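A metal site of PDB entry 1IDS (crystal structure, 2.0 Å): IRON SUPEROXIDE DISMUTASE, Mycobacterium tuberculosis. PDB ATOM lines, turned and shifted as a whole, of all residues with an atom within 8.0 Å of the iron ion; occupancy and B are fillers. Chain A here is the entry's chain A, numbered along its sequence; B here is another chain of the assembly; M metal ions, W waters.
The side-chain carboxylate of Asp 160 sits at hydrogen-bond distance from the backbone NH of Trp 162 (3.0 Å).
A ring nitrogen (ND1) of His 76 is in hydrogen-bond range of the backbone carbonyl oxygen (O) of Gly 72 (2.7 Å).
The backbone carbonyl oxygen (O) of His 76 sits close to the indole nitrogen (NE1) of Trp 80.
ND1 of His 164 lies within hydrogen-bond range of OE2 of Glu 163 of chain B (2.7 Å).
N of His 33 lies within hydrogen-bond range of O of His 28, 2.9 Å away.
Water W1 bridges the side-chain carboxylate (OD1) of Asp 160 (2.8 Å) and the indole nitrogen (NE1) of Trp 162 (3.4 Å).
Four residues have an atom within 4 Å of the iron ion: His 28, His 76, Asp 160 and His 164.
The iron ion is bound by OD2 of Asp 160 (2.0 Å), NE2 of His 76 (2.2 Å), NE2 of His 164 (2.2 Å), NE2 of His 28 (2.3 Å) and water W1 (2.4 Å).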
ATOM      1  N   HIS A  28      -6.060 -12.496  -2.409  1.00  0.00           N
ATOM      2  CA  HIS A  28      -6.368 -11.122  -2.793  1.00  0.00           C
ATOM      3  C   HIS A  28      -7.767 -10.982  -3.365  1.00  0.00           C
ATOM      4  O   HIS A  28      -8.556 -10.140  -2.958  1.00  0.00           O
ATOM      5  CB  HIS A  28      -5.363 -10.630  -3.832  1.00  0.00           C
ATOM      6  CG  HIS A  28      -5.179  -9.113  -3.821  1.00  0.00           C
ATOM      7  ND1 HIS A  28      -4.344  -8.439  -4.710  1.00  0.00           N
ATOM      8  CD2 HIS A  28      -5.775  -8.193  -2.995  1.00  0.00           C
ATOM      9  CE1 HIS A  28      -4.414  -7.081  -4.422  1.00  0.00           C
ATOM     10  NE2 HIS A  28      -5.286  -6.947  -3.353  1.00  0.00           N
ATOM     11  N   HIS A  29      -8.070 -11.804  -4.338  1.00  0.00           N
ATOM     12  CA  HIS A  29      -9.346 -11.826  -5.031  1.00  0.00           C
ATOM     13  C   HIS A  29     -10.453 -12.453  -4.218  1.00  0.00           C
ATOM     14  O   HIS A  29     -11.450 -11.811  -3.915  1.00  0.00           O
ATOM     15  CB  HIS A  29      -9.211 -12.608  -6.352  1.00  0.00           C
ATOM     16  CG  HIS A  29     -10.519 -12.653  -7.155  1.00  0.00           C
ATOM     17  ND1 HIS A  29     -11.330 -13.768  -7.313  1.00  0.00           N
ATOM     18  CD2 HIS A  29     -11.073 -11.590  -7.852  1.00  0.00           C
ATOM     19  CE1 HIS A  29     -12.398 -13.400  -8.109  1.00  0.00           C
ATOM     20  NE2 HIS A  29     -12.243 -12.060  -8.449  1.00  0.00           N
ATOM     21  N   HIS A  32      -9.894 -10.824   0.238  1.00  0.00           N
ATOM     22  CA  HIS A  32      -9.836  -9.379   0.397  1.00  0.00           C
ATOM     23  C   HIS A  32     -10.860  -8.645  -0.423  1.00  0.00           C
ATOM     24  O   HIS A  32     -11.681  -7.897   0.091  1.00  0.00           O
ATOM     25  CB  HIS A  32      -8.440  -8.843   0.054  1.00  0.00           C
ATOM     26  CG  HIS A  32      -7.400  -9.313   1.068  1.00  0.00           C
ATOM     27  ND1 HIS A  32      -7.260  -8.797   2.343  1.00  0.00           N
ATOM     28  CD2 HIS A  32      -6.447 -10.309   0.874  1.00  0.00           C
ATOM     29  CE1 HIS A  32      -6.210  -9.461   2.964  1.00  0.00           C
ATOM     30  NE2 HIS A  32      -5.721 -10.389   2.048  1.00  0.00           N
ATOM     31  N   HIS A  33     -10.825  -8.811  -1.749  1.00  0.00           N
ATOM     32  CA  HIS A  33     -11.781  -8.126  -2.618  1.00  0.00           C
ATOM     33  C   HIS A  33     -13.223  -8.470  -2.234  1.00  0.00           C
ATOM     34  O   HIS A  33     -14.069  -7.581  -2.173  1.00  0.00           O
ATOM     35  CB  HIS A  33     -11.546  -8.504  -4.078  1.00  0.00           C
ATOM     36  CG  HIS A  33     -12.257  -7.546  -5.037  1.00  0.00           C
ATOM     37  ND1 HIS A  33     -12.011  -7.466  -6.408  1.00  0.00           N
ATOM     38  CD2 HIS A  33     -13.226  -6.617  -4.708  1.00  0.00           C
ATOM     39  CE1 HIS A  33     -12.844  -6.493  -6.940  1.00  0.00           C
ATOM     40  NE2 HIS A  33     -13.584  -5.970  -5.883  1.00  0.00           N
ATOM     41  N   TYR A  36     -14.581  -6.487   0.584  1.00  0.00           N
ATOM     42  CA  TYR A  36     -14.934  -5.094   0.230  1.00  0.00           C
ATOM     43  C   TYR A  36     -16.292  -5.073  -0.465  1.00  0.00           C
ATOM     44  O   TYR A  36     -17.062  -4.130  -0.279  1.00  0.00           O
ATOM     45  CB  TYR A  36     -13.884  -4.438  -0.619  1.00  0.00           C
ATOM     46  CG  TYR A  36     -12.522  -4.290   0.042  1.00  0.00           C
ATOM     47  CD1 TYR A  36     -12.409  -3.724   1.310  1.00  0.00           C
ATOM     48  CD2 TYR A  36     -11.360  -4.715  -0.615  1.00  0.00           C
ATOM     49  CE1 TYR A  36     -11.157  -3.593   1.898  1.00  0.00           C
ATOM     50  CE2 TYR A  36     -10.122  -4.581  -0.018  1.00  0.00           C
ATOM     51  CZ  TYR A  36     -10.007  -4.011   1.241  1.00  0.00           C
ATOM     52  OH  TYR A  36      -8.779  -3.878   1.835  1.00  0.00           O
ATOM     53  N   GLY A  72     -12.653   0.458  -1.851  1.00  0.00           N
ATOM     54  CA  GLY A  72     -11.903  -0.815  -1.854  1.00  0.00           C
ATOM     55  C   GLY A  72     -12.321  -1.644  -3.078  1.00  0.00           C
ATOM     56  O   GLY A  72     -11.489  -2.158  -3.822  1.00  0.00           O
ATOM     57  N   ASN A  75     -11.247   0.135  -6.559  1.00  0.00           N
ATOM     58  CA  ASN A  75      -9.811   0.024  -6.803  1.00  0.00           C
ATOM     59  C   ASN A  75      -9.397  -1.367  -7.259  1.00  0.00           C
ATOM     60  O   ASN A  75      -8.534  -1.467  -8.134  1.00  0.00           O
ATOM     61  CB  ASN A  75      -9.005   0.365  -5.537  1.00  0.00           C
ATOM     62  CG  ASN A  75      -9.189   1.834  -5.162  1.00  0.00           C
ATOM     63  OD1 ASN A  75      -9.927   2.640  -5.915  1.00  0.00           O
ATOM     64  ND2 ASN A  75      -8.612   2.319  -4.076  1.00  0.00           N
ATOM     65  N   HIS A  76      -9.922  -2.421  -6.675  1.00  0.00           N
ATOM     66  CA  HIS A  76      -9.564  -3.797  -7.039  1.00  0.00           C
ATOM     67  C   HIS A  76     -10.166  -4.212  -8.361  1.00  0.00           C
ATOM     68  O   HIS A  76      -9.524  -4.950  -9.102  1.00  0.00           O
ATOM     69  CB  HIS A  76     -10.016  -4.768  -5.942  1.00  0.00           C
ATOM     70  CG  HIS A  76      -9.124  -4.609  -4.714  1.00  0.00           C
ATOM     71  ND1 HIS A  76      -9.410  -3.812  -3.610  1.00  0.00           N
ATOM     72  CD2 HIS A  76      -7.899  -5.213  -4.494  1.00  0.00           C
ATOM     73  CE1 HIS A  76      -8.371  -3.921  -2.702  1.00  0.00           C
ATOM     74  NE2 HIS A  76      -7.442  -4.789  -3.253  1.00  0.00           N
ATOM     75  N   TRP A  79      -7.934  -2.901 -10.829  1.00  0.00           N
ATOM     76  CA  TRP A  79      -6.653  -3.617 -10.622  1.00  0.00           C
ATOM     77  C   TRP A  79      -6.623  -4.897 -11.441  1.00  0.00           C
ATOM     78  O   TRP A  79      -5.649  -5.073 -12.172  1.00  0.00           O
ATOM     79  CB  TRP A  79      -6.440  -3.898  -9.149  1.00  0.00           C
ATOM     80  CG  TRP A  79      -5.347  -4.877  -8.774  1.00  0.00           C
ATOM     81  CD1 TRP A  79      -5.562  -6.128  -8.274  1.00  0.00           C
ATOM     82  CD2 TRP A  79      -3.965  -4.674  -8.831  1.00  0.00           C
ATOM     83  NE1 TRP A  79      -4.284  -6.701  -8.036  1.00  0.00           N
ATOM     84  CE2 TRP A  79      -3.356  -5.832  -8.367  1.00  0.00           C
ATOM     85  CE3 TRP A  79      -3.140  -3.621  -9.231  1.00  0.00           C
ATOM     86  CZ2 TRP A  79      -2.016  -5.981  -8.292  1.00  0.00           C
ATOM     87  CZ3 TRP A  79      -1.764  -3.766  -9.167  1.00  0.00           C
ATOM     88  CH2 TRP A  79      -1.188  -4.950  -8.689  1.00  0.00           C
ATOM     89  N   TRP A  80      -7.634  -5.748 -11.340  1.00  0.00           N
ATOM     90  CA  TRP A  80      -7.710  -7.013 -12.079  1.00  0.00           C
ATOM     91  C   TRP A  80      -7.668  -6.778 -13.583  1.00  0.00           C
ATOM     92  O   TRP A  80      -7.063  -7.589 -14.276  1.00  0.00           O
ATOM     93  CB  TRP A  80      -8.966  -7.794 -11.742  1.00  0.00           C
ATOM     94  CG  TRP A  80      -9.106  -8.094 -10.262  1.00  0.00           C
ATOM     95  CD1 TRP A  80     -10.167  -7.817  -9.486  1.00  0.00           C
ATOM     96  CD2 TRP A  80      -8.113  -8.705  -9.473  1.00  0.00           C
ATOM     97  NE1 TRP A  80      -9.837  -8.269  -8.173  1.00  0.00           N
ATOM     98  CE2 TRP A  80      -8.628  -8.788  -8.190  1.00  0.00           C
ATOM     99  CE3 TRP A  80      -6.835  -9.217  -9.719  1.00  0.00           C
ATOM    100  CZ2 TRP A  80      -7.930  -9.340  -7.172  1.00  0.00           C
ATOM    101  CZ3 TRP A  80      -6.114  -9.773  -8.673  1.00  0.00           C
ATOM    102  CH2 TRP A  80      -6.660  -9.838  -7.402  1.00  0.00           C
ATOM    103  N   GLY A 124      -1.998   2.070   0.899  1.00  0.00           N
ATOM    104  CA  GLY A 124      -2.332   3.034  -0.158  1.00  0.00           C
ATOM    105  C   GLY A 124      -2.099   2.423  -1.532  1.00  0.00           C
ATOM    106  O   GLY A 124      -1.707   1.274  -1.646  1.00  0.00           O
ATOM    107  N   TRP A 125      -2.308   3.241  -2.542  1.00  0.00           N
ATOM    108  CA  TRP A 125      -2.155   2.889  -3.932  1.00  0.00           C
ATOM    109  C   TRP A 125      -1.475   4.063  -4.679  1.00  0.00           C
ATOM    110  O   TRP A 125      -1.395   5.190  -4.219  1.00  0.00           O
ATOM    111  CB  TRP A 125      -3.501   2.663  -4.636  1.00  0.00           C
ATOM    112  CG  TRP A 125      -4.496   1.656  -4.081  1.00  0.00           C
ATOM    113  CD1 TRP A 125      -5.072   1.703  -2.868  1.00  0.00           C
ATOM    114  CD2 TRP A 125      -4.985   0.528  -4.746  1.00  0.00           C
ATOM    115  NE1 TRP A 125      -5.930   0.574  -2.763  1.00  0.00           N
ATOM    116  CE2 TRP A 125      -5.873  -0.110  -3.878  1.00  0.00           C
ATOM    117  CE3 TRP A 125      -4.784  -0.055  -6.014  1.00  0.00           C
ATOM    118  CZ2 TRP A 125      -6.534  -1.236  -4.182  1.00  0.00           C
ATOM    119  CZ3 TRP A 125      -5.469  -1.221  -6.321  1.00  0.00           C
ATOM    120  CH2 TRP A 125      -6.342  -1.822  -5.420  1.00  0.00           C
ATOM    121  N   HIS A 145      -7.976   3.543   0.749  1.00  0.00           N
ATOM    122  CA  HIS A 145      -8.571   3.300  -0.583  1.00  0.00           C
ATOM    123  C   HIS A 145      -9.312   4.567  -1.057  1.00  0.00           C
ATOM    124  O   HIS A 145      -9.510   4.748  -2.254  1.00  0.00           O
ATOM    125  CB  HIS A 145      -9.712   2.239  -0.410  1.00  0.00           C
ATOM    126  CG  HIS A 145      -9.184   0.822  -0.235  1.00  0.00           C
ATOM    127  ND1 HIS A 145      -8.171   0.224  -0.967  1.00  0.00           N
ATOM    128  CD2 HIS A 145      -9.664  -0.099   0.707  1.00  0.00           C
ATOM    129  CE1 HIS A 145      -8.019  -1.066  -0.486  1.00  0.00           C
ATOM    130  NE2 HIS A 145      -8.928  -1.257   0.537  1.00  0.00           N
ATOM    131  N   LEU A 159      -1.948   0.772  -8.867  1.00  0.00           N
ATOM    132  CA  LEU A 159      -0.905  -0.062  -8.269  1.00  0.00           C
ATOM    133  C   LEU A 159      -1.226  -0.226  -6.765  1.00  0.00           C
ATOM    134  O   LEU A 159      -1.085   0.715  -5.998  1.00  0.00           O
ATOM    135  CB  LEU A 159       0.471   0.480  -8.467  1.00  0.00           C
ATOM    136  CG  LEU A 159       1.599  -0.325  -7.878  1.00  0.00           C
ATOM    137  CD1 LEU A 159       1.493  -1.819  -8.152  1.00  0.00           C
ATOM    138  CD2 LEU A 159       2.990   0.163  -8.245  1.00  0.00           C
ATOM    139  N   ASP A 160      -1.674  -1.408  -6.400  1.00  0.00           N
ATOM    140  CA  ASP A 160      -2.023  -1.749  -5.008  1.00  0.00           C
ATOM    141  C   ASP A 160      -0.753  -1.819  -4.166  1.00  0.00           C
ATOM    142  O   ASP A 160       0.147  -2.604  -4.460  1.00  0.00           O
ATOM    143  CB  ASP A 160      -2.774  -3.065  -4.970  1.00  0.00           C
ATOM    144  CG  ASP A 160      -3.424  -3.314  -3.619  1.00  0.00           C
ATOM    145  OD1 ASP A 160      -3.254  -2.504  -2.688  1.00  0.00           O
ATOM    146  OD2 ASP A 160      -4.124  -4.335  -3.498  1.00  0.00           O
ATOM    147  N   MET A 161      -0.625  -0.985  -3.157  1.00  0.00           N
ATOM    148  CA  MET A 161       0.532  -0.929  -2.266  1.00  0.00           C
ATOM    149  C   MET A 161       0.164  -1.367  -0.867  1.00  0.00           C
ATOM    150  O   MET A 161       0.905  -1.127   0.084  1.00  0.00           O
ATOM    151  CB  MET A 161       1.239   0.397  -2.278  1.00  0.00           C
ATOM    152  CG  MET A 161       1.916   0.688  -3.602  1.00  0.00           C
ATOM    153  SD  MET A 161       3.045  -0.650  -4.132  1.00  0.00           S
ATOM    154  CE  MET A 161       4.436  -0.706  -2.966  1.00  0.00           C
ATOM    155  N   TRP A 162      -0.988  -2.004  -0.741  1.00  0.00           N
ATOM    156  CA  TRP A 162      -1.383  -2.513   0.618  1.00  0.00           C
ATOM    157  C   TRP A 162      -0.401  -3.696   0.857  1.00  0.00           C
ATOM    158  O   TRP A 162      -0.060  -4.339  -0.139  1.00  0.00           O
ATOM    159  CB  TRP A 162      -2.789  -2.995   0.631  1.00  0.00           C
ATOM    160  CG  TRP A 162      -3.838  -1.926   0.878  1.00  0.00           C
ATOM    161  CD1 TRP A 162      -3.999  -0.794   0.162  1.00  0.00           C
ATOM    162  CD2 TRP A 162      -4.809  -1.935   1.899  1.00  0.00           C
ATOM    163  NE1 TRP A 162      -5.094  -0.073   0.735  1.00  0.00           N
ATOM    164  CE2 TRP A 162      -5.564  -0.763   1.752  1.00  0.00           C
ATOM    165  CE3 TRP A 162      -5.158  -2.807   2.933  1.00  0.00           C
ATOM    166  CZ2 TRP A 162      -6.595  -0.437   2.570  1.00  0.00           C
ATOM    167  CZ3 TRP A 162      -6.227  -2.476   3.766  1.00  0.00           C
ATOM    168  CH2 TRP A 162      -6.953  -1.298   3.596  1.00  0.00           C
ATOM    169  N   GLU A 163       0.057  -3.914   2.063  1.00  0.00           N
ATOM    170  CA  GLU A 163       0.994  -4.983   2.376  1.00  0.00           C
ATOM    171  C   GLU A 163       0.532  -6.337   1.920  1.00  0.00           C
ATOM    172  O   GLU A 163       1.339  -7.189   1.525  1.00  0.00           O
ATOM    173  CB  GLU A 163       1.352  -4.977   3.851  1.00  0.00           C
ATOM    174  CG  GLU A 163       2.514  -4.020   4.091  1.00  0.00           C
ATOM    175  CD  GLU A 163       2.741  -3.742   5.565  1.00  0.00           C
ATOM    176  OE1 GLU A 163       1.871  -3.989   6.413  1.00  0.00           O
ATOM    177  OE2 GLU A 163       3.830  -3.241   5.926  1.00  0.00           O
ATOM    178  N   HIS A 164      -0.755  -6.613   1.925  1.00  0.00           N
ATOM    179  CA  HIS A 164      -1.295  -7.906   1.510  1.00  0.00           C
ATOM    180  C   HIS A 164      -1.167  -8.135   0.010  1.00  0.00           C
ATOM    181  O   HIS A 164      -1.452  -9.203  -0.503  1.00  0.00           O
ATOM    182  CB  HIS A 164      -2.752  -8.074   1.915  1.00  0.00           C
ATOM    183  CG  HIS A 164      -3.702  -7.139   1.185  1.00  0.00           C
ATOM    184  ND1 HIS A 164      -4.611  -6.280   1.805  1.00  0.00           N
ATOM    185  CD2 HIS A 164      -3.833  -6.983  -0.187  1.00  0.00           C
ATOM    186  CE1 HIS A 164      -5.300  -5.593   0.818  1.00  0.00           C
ATOM    187  NE2 HIS A 164      -4.823  -6.027  -0.419  1.00  0.00           N
ATOM    188  N   ALA A 165      -0.742  -7.106  -0.704  1.00  0.00           N
ATOM    189  CA  ALA A 165      -0.595  -7.236  -2.154  1.00  0.00           C
ATOM    190  C   ALA A 165       0.736  -7.849  -2.532  1.00  0.00           C
ATOM    191  O   ALA A 165       0.847  -8.392  -3.625  1.00  0.00           O
ATOM    192  CB  ALA A 165      -0.752  -5.872  -2.807  1.00  0.00           C
ATOM    193  N   PHE A 166       1.735  -7.780  -1.656  1.00  0.00           N
ATOM    194  CA  PHE A 166       3.044  -8.335  -2.060  1.00  0.00           C
ATOM    195  C   PHE A 166       3.780  -9.028  -0.961  1.00  0.00           C
ATOM    196  O   PHE A 166       4.816  -9.663  -1.193  1.00  0.00           O
ATOM    197  CB  PHE A 166       3.924  -7.152  -2.555  1.00  0.00           C
ATOM    198  CG  PHE A 166       4.080  -6.085  -1.464  1.00  0.00           C
ATOM    199  CD1 PHE A 166       5.058  -6.227  -0.487  1.00  0.00           C
ATOM    200  CD2 PHE A 166       3.244  -4.965  -1.419  1.00  0.00           C
ATOM    201  CE1 PHE A 166       5.224  -5.288   0.513  1.00  0.00           C
ATOM    202  CE2 PHE A 166       3.418  -4.029  -0.407  1.00  0.00           C
ATOM    203  CZ  PHE A 166       4.401  -4.176   0.558  1.00  0.00           C
ATOM    204  N   GLU B 163      -0.695  -5.402   8.446  1.00  0.00           N
ATOM    205  CA  GLU B 163      -0.619  -6.677   7.767  1.00  0.00           C
ATOM    206  C   GLU B 163       0.673  -7.401   7.917  1.00  0.00           C
ATOM    207  O   GLU B 163       0.696  -8.626   8.063  1.00  0.00           O
ATOM    208  CB  GLU B 163      -1.049  -6.560   6.317  1.00  0.00           C
ATOM    209  CG  GLU B 163      -2.510  -6.150   6.249  1.00  0.00           C
ATOM    210  CD  GLU B 163      -2.977  -6.023   4.805  1.00  0.00           C
ATOM    211  OE1 GLU B 163      -2.273  -5.467   3.950  1.00  0.00           O
ATOM    212  OE2 GLU B 163      -4.086  -6.477   4.482  1.00  0.00           O
HETATM  213 FE    FE M   1      -5.508  -4.999  -2.247  1.00  0.00          FE
HETATM  214  O   HOH W   1      -5.611  -2.875  -1.162  1.00  0.00           O
